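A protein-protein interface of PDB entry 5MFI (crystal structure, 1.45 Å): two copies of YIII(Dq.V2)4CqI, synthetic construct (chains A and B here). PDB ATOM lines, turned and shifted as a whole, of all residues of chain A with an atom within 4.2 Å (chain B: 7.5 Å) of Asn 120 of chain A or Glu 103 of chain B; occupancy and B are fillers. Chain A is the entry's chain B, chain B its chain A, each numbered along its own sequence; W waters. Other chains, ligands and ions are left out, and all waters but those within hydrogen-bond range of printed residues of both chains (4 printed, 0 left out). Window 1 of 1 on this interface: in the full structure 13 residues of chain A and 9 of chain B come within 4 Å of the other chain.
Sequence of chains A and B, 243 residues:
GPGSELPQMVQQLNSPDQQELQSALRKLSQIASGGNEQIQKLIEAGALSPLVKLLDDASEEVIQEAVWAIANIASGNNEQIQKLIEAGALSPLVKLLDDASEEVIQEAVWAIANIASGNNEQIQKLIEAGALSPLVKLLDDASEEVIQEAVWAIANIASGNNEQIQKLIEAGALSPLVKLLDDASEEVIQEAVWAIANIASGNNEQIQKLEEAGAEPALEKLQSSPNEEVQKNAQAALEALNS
N of Asn 120 of chain A sits at hydrogen-bond distance from OE1 of Glu 103 of chain B (3.0 Å).
The side-chain hydroxyl (OG) of Ser 101 of chain B is in hydrogen-bond range of the side-chain carboxylate (OE2) of Glu 60 of chain B. The backbone NH (N) of Val 104 of chain B lies within hydrogen-bond range of the side-chain hydroxyl (OG) of Ser 101 of chain B (3.2 Å). The side-chain amide oxygen of Asn 119 of chain A lies within hydrogen-bond range of the backbone NH of Glu 121 of chain A. N of Asn 119 of chain A sits at hydrogen-bond distance from OE1 of Gln 122 of chain A, at 2.9 Å. O of Asn 120 of chain A sits at hydrogen-bond distance from NE2 of Gln 164 of chain A (2.8 Å). The side-chain amide oxygen of Gln 164 of chain A is in hydrogen-bond range of the backbone NH of Asn 161 of chain A (2.9 Å).
Among the printed residues, merely in contact across the chains: Asn 161 of chain A with Glu 145 of chain B, Asn 119 of chain A with Glu 103 of chain B and Glu 121 of chain A with Ser 101 of chain B.
Asn 120 of chain A touches one residue of chain B. Glu 103 of chain B touches just these residues of chain A: Asn 119 and Asn 120. Of the printed residues of chain B, Asn 119 of chain A touches Glu 103 (3.5 Å). Of the printed residues of chain B, Asn 161 of chain A touches Glu 145. Printed residues of chain B within 4 Å of Glu 121 of chain A: Ser 101. Of the printed residues of chain A, Ser 101 of chain B touches Glu 121. Of the printed residues of chain A, Glu 145 of chain B touches Asn 161. Glu 60 of chain B touches none of the printed residues of chain A.
Of the 10 printed residues of chain A, 4 touch a printed residue of chain B. Printed residues of chain A that touch a printed residue of chain B: Asn 119, Asn 120, Glu 121 and Asn 161. Along chain A the printed residues that touch a printed residue of chain B span positions 119 to 161. Among the printed residues, no Asp or Glu carboxylate lies within 4 Å of a Lys or Arg side-chain nitrogen of the other chain.
No position is printed for both chains. Of the 4 pairs that touch across the chains among the printed residues, none has its exchanged pair printed and touching as well.
Water W1 bridges the side-chain carboxylate (OE2) of Glu 121 of chain A (2.7 Å) and the backbone NH (N) of Glu 102 of chain B (2.9 Å). Water W4 lies within hydrogen-bond range of the side-chain carboxylate of Glu 60 of chain B (2.7 Å) and the side-chain amide nitrogen of Asn 119 of chain A (3.2 Å). Water W2 lies within hydrogen-bond range of OE1 of Glu 103 of chain B (2.7 Å), N of Asn 120 of chain A (3.3 Å) and N of Glu 121 of chain A (3.3 Å). Water W3 bridges NE2 of Gln 106 of chain B and ND2 of Asn 120 of chain A.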
ATOM      1  N   GLY A 118     -20.802   6.136 -17.972  1.00  0.00           N
ATOM      2  CA  GLY A 118     -20.364   5.384 -16.810  1.00  0.00           C
ATOM      3  C   GLY A 118     -18.853   5.342 -16.713  1.00  0.00           C
ATOM      4  O   GLY A 118     -18.149   6.174 -17.308  1.00  0.00           O
ATOM      5  N   ASN A 119     -18.339   4.382 -15.940  1.00  0.00           N
ATOM      6  CA  ASN A 119     -16.895   4.276 -15.767  1.00  0.00           C
ATOM      7  C   ASN A 119     -16.253   3.587 -16.983  1.00  0.00           C
ATOM      8  O   ASN A 119     -16.963   3.053 -17.842  1.00  0.00           O
ATOM      9  CB  ASN A 119     -16.538   3.593 -14.451  1.00  0.00           C
ATOM     10  CG  ASN A 119     -17.016   2.170 -14.345  1.00  0.00           C
ATOM     11  OD1 ASN A 119     -16.797   1.349 -15.243  1.00  0.00           O
ATOM     12  ND2 ASN A 119     -17.626   1.833 -13.218  1.00  0.00           N
ATOM     13  N   ASN A 120     -14.903   3.579 -17.048  1.00  0.00           N
ATOM     14  CA  ASN A 120     -14.211   2.976 -18.185  1.00  0.00           C
ATOM     15  C   ASN A 120     -14.436   1.480 -18.348  1.00  0.00           C
ATOM     16  O   ASN A 120     -14.430   1.004 -19.484  1.00  0.00           O
ATOM     17  CB  ASN A 120     -12.736   3.291 -18.110  1.00  0.00           C
ATOM     18  CG  ASN A 120     -12.453   4.759 -18.314  1.00  0.00           C
ATOM     19  OD1 ASN A 120     -13.354   5.554 -18.624  1.00  0.00           O
ATOM     20  ND2 ASN A 120     -11.199   5.164 -18.098  1.00  0.00           N
ATOM     21  N   GLU A 121     -14.661   0.737 -17.244  1.00  0.00           N
ATOM     22  CA  GLU A 121     -14.959  -0.689 -17.349  1.00  0.00           C
ATOM     23  C   GLU A 121     -16.311  -0.866 -18.037  1.00  0.00           C
ATOM     24  O   GLU A 121     -16.503  -1.839 -18.764  1.00  0.00           O
ATOM     25  CB  GLU A 121     -14.970  -1.359 -15.979  1.00  0.00           C
ATOM     26  CG  GLU A 121     -13.587  -1.368 -15.348  1.00  0.00           C
ATOM     27  CD  GLU A 121     -13.475  -2.085 -14.017  1.00  0.00           C
ATOM     28  OE1 GLU A 121     -14.524  -2.443 -13.435  1.00  0.00           O
ATOM     29  OE2 GLU A 121     -12.330  -2.282 -13.551  1.00  0.00           O
ATOM     30  N   GLN A 122     -17.233   0.100 -17.839  1.00  0.00           N
ATOM     31  CA  GLN A 122     -18.554   0.044 -18.461  1.00  0.00           C
ATOM     32  C   GLN A 122     -18.466   0.397 -19.955  1.00  0.00           C
ATOM     33  O   GLN A 122     -19.121  -0.247 -20.781  1.00  0.00           O
ATOM     34  CB  GLN A 122     -19.531   0.941 -17.706  1.00  0.00           C
ATOM     35  CG  GLN A 122     -19.818   0.351 -16.331  1.00  0.00           C
ATOM     36  CD  GLN A 122     -20.579   1.253 -15.395  1.00  0.00           C
ATOM     37  OE1 GLN A 122     -20.476   2.482 -15.451  1.00  0.00           O
ATOM     38  NE2 GLN A 122     -21.279   0.630 -14.450  1.00  0.00           N
ATOM     39  N   ILE A 123     -17.589   1.364 -20.302  1.00  0.00           N
ATOM     40  CA  ILE A 123     -17.345   1.689 -21.708  1.00  0.00           C
ATOM     41  C   ILE A 123     -16.745   0.431 -22.367  1.00  0.00           C
ATOM     42  O   ILE A 123     -17.103   0.096 -23.492  1.00  0.00           O
ATOM     43  CB  ILE A 123     -16.389   2.907 -21.849  1.00  0.00           C
ATOM     44  CG1 ILE A 123     -17.058   4.222 -21.386  1.00  0.00           C
ATOM     45  CG2 ILE A 123     -15.857   3.044 -23.293  1.00  0.00           C
ATOM     46  CD1 ILE A 123     -16.041   5.445 -21.250  1.00  0.00           C
ATOM     47  N   GLN A 124     -15.840  -0.277 -21.655  1.00  0.00           N
ATOM     48  CA  GLN A 124     -15.240  -1.485 -22.211  1.00  0.00           C
ATOM     49  C   GLN A 124     -16.309  -2.533 -22.552  1.00  0.00           C
ATOM     50  O   GLN A 124     -16.216  -3.181 -23.596  1.00  0.00           O
ATOM     51  CB  GLN A 124     -14.197  -2.072 -21.241  1.00  0.00           C
ATOM     52  CG  GLN A 124     -13.353  -3.204 -21.832  1.00  0.00           C
ATOM     53  CD  GLN A 124     -12.599  -2.802 -23.078  1.00  0.00           C
ATOM     54  OE1 GLN A 124     -12.258  -1.633 -23.286  1.00  0.00           O
ATOM     55  NE2 GLN A 124     -12.369  -3.757 -23.958  1.00  0.00           N
ATOM     56  N   GLY A 160     -13.054   7.813 -22.386  1.00  0.00           N
ATOM     57  CA  GLY A 160     -12.454   6.632 -21.784  1.00  0.00           C
ATOM     58  C   GLY A 160     -10.942   6.685 -21.857  1.00  0.00           C
ATOM     59  O   GLY A 160     -10.367   7.746 -22.109  1.00  0.00           O
ATOM     60  N   ASN A 161     -10.281   5.546 -21.624  1.00  0.00           N
ATOM     61  CA  ASN A 161      -8.814   5.505 -21.653  1.00  0.00           C
ATOM     62  C   ASN A 161      -8.265   5.491 -23.085  1.00  0.00           C
ATOM     63  O   ASN A 161      -9.036   5.386 -24.050  1.00  0.00           O
ATOM     64  CB  ASN A 161      -8.284   4.323 -20.825  1.00  0.00           C
ATOM     65  CG  ASN A 161      -8.705   2.959 -21.327  1.00  0.00           C
ATOM     66  OD1 ASN A 161      -8.566   2.640 -22.514  1.00  0.00           O
ATOM     67  ND2 ASN A 161      -9.170   2.101 -20.417  1.00  0.00           N
ATOM     68  N   GLN A 164      -9.272   2.643 -25.384  1.00  0.00           N
ATOM     69  CA  GLN A 164     -10.648   2.789 -25.844  1.00  0.00           C
ATOM     70  C   GLN A 164     -10.716   3.790 -26.992  1.00  0.00           C
ATOM     71  O   GLN A 164     -11.425   3.543 -27.969  1.00  0.00           O
ATOM     72  CB  GLN A 164     -11.579   3.121 -24.674  1.00  0.00           C
ATOM     73  CG  GLN A 164     -11.613   1.951 -23.675  1.00  0.00           C
ATOM     74  CD  GLN A 164     -12.276   2.270 -22.364  1.00  0.00           C
ATOM     75  OE1 GLN A 164     -12.233   3.402 -21.876  1.00  0.00           O
ATOM     76  NE2 GLN A 164     -12.866   1.258 -21.736  1.00  0.00           N
ATOM     77  N   GLU B  60     -17.227   3.287  -5.921  1.00  0.00           N
ATOM     78  CA  GLU B  60     -16.250   3.493  -7.002  1.00  0.00           C
ATOM     79  C   GLU B  60     -16.430   4.863  -7.672  1.00  0.00           C
ATOM     80  O   GLU B  60     -15.441   5.544  -7.965  1.00  0.00           O
ATOM     81  CB  GLU B  60     -16.367   2.356  -8.052  1.00  0.00           C
ATOM     82  CG  GLU B  60     -15.664   2.580  -9.392  1.00  0.00           C
ATOM     83  CD  GLU B  60     -14.148   2.505  -9.418  1.00  0.00           C
ATOM     84  OE1 GLU B  60     -13.549   2.220  -8.359  1.00  0.00           O
ATOM     85  OE2 GLU B  60     -13.557   2.705 -10.505  1.00  0.00           O
ATOM     86  N   GLN B  64     -13.606   7.780  -7.691  1.00  0.00           N
ATOM     87  CA  GLN B  64     -13.062   8.338  -8.941  1.00  0.00           C
ATOM     88  C   GLN B  64     -13.079   9.865  -8.920  1.00  0.00           C
ATOM     89  O   GLN B  64     -12.072  10.484  -9.264  1.00  0.00           O
ATOM     90  CB  GLN B  64     -13.806   7.799 -10.174  1.00  0.00           C
ATOM     91  CG  GLN B  64     -13.201   8.207 -11.540  1.00  0.00           C
ATOM     92  CD  GLN B  64     -13.560   9.608 -12.035  1.00  0.00           C
ATOM     93  OE1 GLN B  64     -12.697  10.417 -12.381  1.00  0.00           O
ATOM     94  NE2 GLN B  64     -14.833   9.942 -12.100  1.00  0.00           N
ATOM     95  N   GLU B  65     -14.203  10.469  -8.504  1.00  0.00           N
ATOM     96  CA  GLU B  65     -14.314  11.924  -8.457  1.00  0.00           C
ATOM     97  C   GLU B  65     -13.439  12.532  -7.356  1.00  0.00           C
ATOM     98  O   GLU B  65     -12.805  13.561  -7.587  1.00  0.00           O
ATOM     99  CB  GLU B  65     -15.779  12.362  -8.300  1.00  0.00           C
ATOM    100  CG  GLU B  65     -16.028  13.791  -8.760  1.00  0.00           C
ATOM    101  CD  GLU B  65     -15.703  14.085 -10.213  1.00  0.00           C
ATOM    102  OE1 GLU B  65     -16.220  13.372 -11.102  1.00  0.00           O
ATOM    103  OE2 GLU B  65     -14.918  15.026 -10.462  1.00  0.00           O
ATOM    104  N   VAL B  67     -10.596  11.278  -6.059  1.00  0.00           N
ATOM    105  CA  VAL B  67      -9.176  11.170  -6.465  1.00  0.00           C
ATOM    106  C   VAL B  67      -8.832  12.241  -7.510  1.00  0.00           C
ATOM    107  O   VAL B  67      -7.746  12.824  -7.447  1.00  0.00           O
ATOM    108  CB  VAL B  67      -8.747   9.742  -6.897  1.00  0.00           C
ATOM    109  CG1 VAL B  67      -7.261   9.689  -7.216  1.00  0.00           C
ATOM    110  CG2 VAL B  67      -9.057   8.724  -5.815  1.00  0.00           C
ATOM    111  N   ALA B 100      -7.462  -1.013  -6.686  1.00  0.00           N
ATOM    112  CA  ALA B 100      -8.389  -0.196  -7.502  1.00  0.00           C
ATOM    113  C   ALA B 100      -8.429  -0.493  -9.027  1.00  0.00           C
ATOM    114  O   ALA B 100      -7.566  -1.192  -9.558  1.00  0.00           O
ATOM    115  CB  ALA B 100      -8.096   1.277  -7.279  1.00  0.00           C
ATOM    116  N   SER B 101      -9.461   0.047  -9.723  1.00  0.00           N
ATOM    117  CA  SER B 101      -9.627  -0.066 -11.179  1.00  0.00           C
ATOM    118  C   SER B 101      -8.490   0.704 -11.862  1.00  0.00           C
ATOM    119  O   SER B 101      -7.915   1.614 -11.253  1.00  0.00           O
ATOM    120  CB  SER B 101     -10.959   0.545 -11.605  1.00  0.00           C
ATOM    121  OG  SER B 101     -11.015   1.921 -11.268  1.00  0.00           O
ATOM    122  N   GLU B 102      -8.199   0.387 -13.138  1.00  0.00           N
ATOM    123  CA  GLU B 102      -7.149   1.089 -13.883  1.00  0.00           C
ATOM    124  C   GLU B 102      -7.454   2.586 -13.972  1.00  0.00           C
ATOM    125  O   GLU B 102      -6.535   3.400 -13.910  1.00  0.00           O
ATOM    126  CB  GLU B 102      -6.953   0.477 -15.279  1.00  0.00           C
ATOM    127  CG  GLU B 102      -5.575   0.729 -15.880  1.00  0.00           C
ATOM    128  CD  GLU B 102      -4.427  -0.178 -15.460  1.00  0.00           C
ATOM    129  OE1 GLU B 102      -3.413  -0.213 -16.196  1.00  0.00           O
ATOM    130  OE2 GLU B 102      -4.527  -0.842 -14.403  1.00  0.00           O
ATOM    131  N   GLU B 103      -8.756   2.947 -14.056  1.00  0.00           N
ATOM    132  CA  GLU B 103      -9.183   4.343 -14.107  1.00  0.00           C
ATOM    133  C   GLU B 103      -8.801   5.068 -12.822  1.00  0.00           C
ATOM    134  O   GLU B 103      -8.239   6.165 -12.887  1.00  0.00           O
ATOM    135  CB  GLU B 103     -10.697   4.425 -14.331  1.00  0.00           C
ATOM    136  CG  GLU B 103     -11.209   5.845 -14.502  1.00  0.00           C
ATOM    137  CD  GLU B 103     -12.683   5.932 -14.846  1.00  0.00           C
ATOM    138  OE1 GLU B 103     -13.343   4.869 -14.897  1.00  0.00           O
ATOM    139  OE2 GLU B 103     -13.181   7.062 -15.048  1.00  0.00           O
ATOM    140  N   VAL B 104      -9.087   4.451 -11.656  1.00  0.00           N
ATOM    141  CA  VAL B 104      -8.759   5.048 -10.353  1.00  0.00           C
ATOM    142  C   VAL B 104      -7.242   5.050 -10.152  1.00  0.00           C
ATOM    143  O   VAL B 104      -6.693   6.075  -9.731  1.00  0.00           O
ATOM    144  CB  VAL B 104      -9.541   4.402  -9.175  1.00  0.00           C
ATOM    145  CG1 VAL B 104      -9.040   4.896  -7.817  1.00  0.00           C
ATOM    146  CG2 VAL B 104     -11.036   4.671  -9.319  1.00  0.00           C
ATOM    147  N   ILE B 105      -6.558   3.932 -10.506  1.00  0.00           N
ATOM    148  CA  ILE B 105      -5.087   3.854 -10.381  1.00  0.00           C
ATOM    149  C   ILE B 105      -4.436   5.004 -11.139  1.00  0.00           C
ATOM    150  O   ILE B 105      -3.615   5.702 -10.552  1.00  0.00           O
ATOM    151  CB  ILE B 105      -4.501   2.467 -10.766  1.00  0.00           C
ATOM    152  CG1 ILE B 105      -4.909   1.385  -9.735  1.00  0.00           C
ATOM    153  CG2 ILE B 105      -2.961   2.517 -10.893  1.00  0.00           C
ATOM    154  CD1 ILE B 105      -4.595  -0.080 -10.198  1.00  0.00           C
ATOM    155  N   GLN B 106      -4.845   5.237 -12.416  1.00  0.00           N
ATOM    156  CA  GLN B 106      -4.289   6.316 -13.242  1.00  0.00           C
ATOM    157  C   GLN B 106      -4.338   7.694 -12.565  1.00  0.00           C
ATOM    158  O   GLN B 106      -3.367   8.451 -12.625  1.00  0.00           O
ATOM    159  CB  GLN B 106      -4.940   6.356 -14.627  1.00  0.00           C
ATOM    160  CG  GLN B 106      -4.044   7.036 -15.650  1.00  0.00           C
ATOM    161  CD  GLN B 106      -4.712   7.263 -16.978  1.00  0.00           C
ATOM    162  OE1 GLN B 106      -4.688   8.376 -17.514  1.00  0.00           O
ATOM    163  NE2 GLN B 106      -5.306   6.217 -17.547  1.00  0.00           N
ATOM    164  N   GLU B 107      -5.454   7.995 -11.899  1.00  0.00           N
ATOM    165  CA  GLU B 107      -5.663   9.252 -11.189  1.00  0.00           C
ATOM    166  C   GLU B 107      -4.850   9.305  -9.909  1.00  0.00           C
ATOM    167  O   GLU B 107      -4.331  10.371  -9.574  1.00  0.00           O
ATOM    168  CB  GLU B 107      -7.136   9.454 -10.876  1.00  0.00           C
ATOM    169  CG  GLU B 107      -8.002   9.543 -12.118  1.00  0.00           C
ATOM    170  CD  GLU B 107      -9.448   9.885 -11.837  1.00  0.00           C
ATOM    171  OE1 GLU B 107      -9.918   9.617 -10.709  1.00  0.00           O
ATOM    172  OE2 GLU B 107     -10.113  10.418 -12.753  1.00  0.00           O
ATOM    173  N   ALA B 108      -4.740   8.176  -9.194  1.00  0.00           N
ATOM    174  CA  ALA B 108      -3.973   8.126  -7.947  1.00  0.00           C
ATOM    175  C   ALA B 108      -2.480   8.331  -8.236  1.00  0.00           C
ATOM    176  O   ALA B 108      -1.819   9.070  -7.502  1.00  0.00           O
ATOM    177  CB  ALA B 108      -4.200   6.796  -7.240  1.00  0.00           C
ATOM    178  N   VAL B 109      -1.973   7.740  -9.346  1.00  0.00           N
ATOM    179  CA  VAL B 109      -0.558   7.904  -9.706  1.00  0.00           C
ATOM    180  C   VAL B 109      -0.295   9.361 -10.151  1.00  0.00           C
ATOM    181  O   VAL B 109       0.756   9.920  -9.837  1.00  0.00           O
ATOM    182  CB  VAL B 109      -0.031   6.816 -10.686  1.00  0.00           C
ATOM    183  CG1 VAL B 109      -0.896   6.669 -11.917  1.00  0.00           C
ATOM    184  CG2 VAL B 109       1.417   7.061 -11.073  1.00  0.00           C
ATOM    185  N   GLU B 145      -0.547   4.249 -20.510  1.00  0.00           N
ATOM    186  CA  GLU B 145      -1.035   5.466 -19.890  1.00  0.00           C
ATOM    187  C   GLU B 145      -0.626   5.569 -18.411  1.00  0.00           C
ATOM    188  O   GLU B 145      -0.193   6.633 -17.976  1.00  0.00           O
ATOM    189  CB  GLU B 145      -2.555   5.491 -20.004  1.00  0.00           C
ATOM    190  CG  GLU B 145      -3.104   6.779 -20.569  1.00  0.00           C
ATOM    191  CD  GLU B 145      -4.615   6.780 -20.641  1.00  0.00           C
ATOM    192  OE1 GLU B 145      -5.197   5.745 -21.041  1.00  0.00           O
ATOM    193  OE2 GLU B 145      -5.219   7.807 -20.261  1.00  0.00           O
ATOM    194  N   VAL B 146      -0.797   4.466 -17.640  1.00  0.00           N
ATOM    195  CA  VAL B 146      -0.459   4.384 -16.213  1.00  0.00           C
ATOM    196  C   VAL B 146       1.072   4.396 -16.067  1.00  0.00           C
ATOM    197  O   VAL B 146       1.588   5.024 -15.147  1.00  0.00           O
ATOM    198  CB  VAL B 146      -1.122   3.163 -15.520  1.00  0.00           C
ATOM    199  CG1 VAL B 146      -0.648   3.003 -14.074  1.00  0.00           C
ATOM    200  CG2 VAL B 146      -2.648   3.274 -15.566  1.00  0.00           C
HETATM  201  O   HOH W   1      -9.949  -1.447 -14.526  1.00  0.00           O
HETATM  202  O   HOH W   2     -13.178   2.143 -14.649  1.00  0.00           O
HETATM  203  O   HOH W   3      -8.115   6.314 -17.524  1.00  0.00           O
HETATM  204  O   HOH W   4     -14.543   1.151 -12.528  1.00  0.00           O
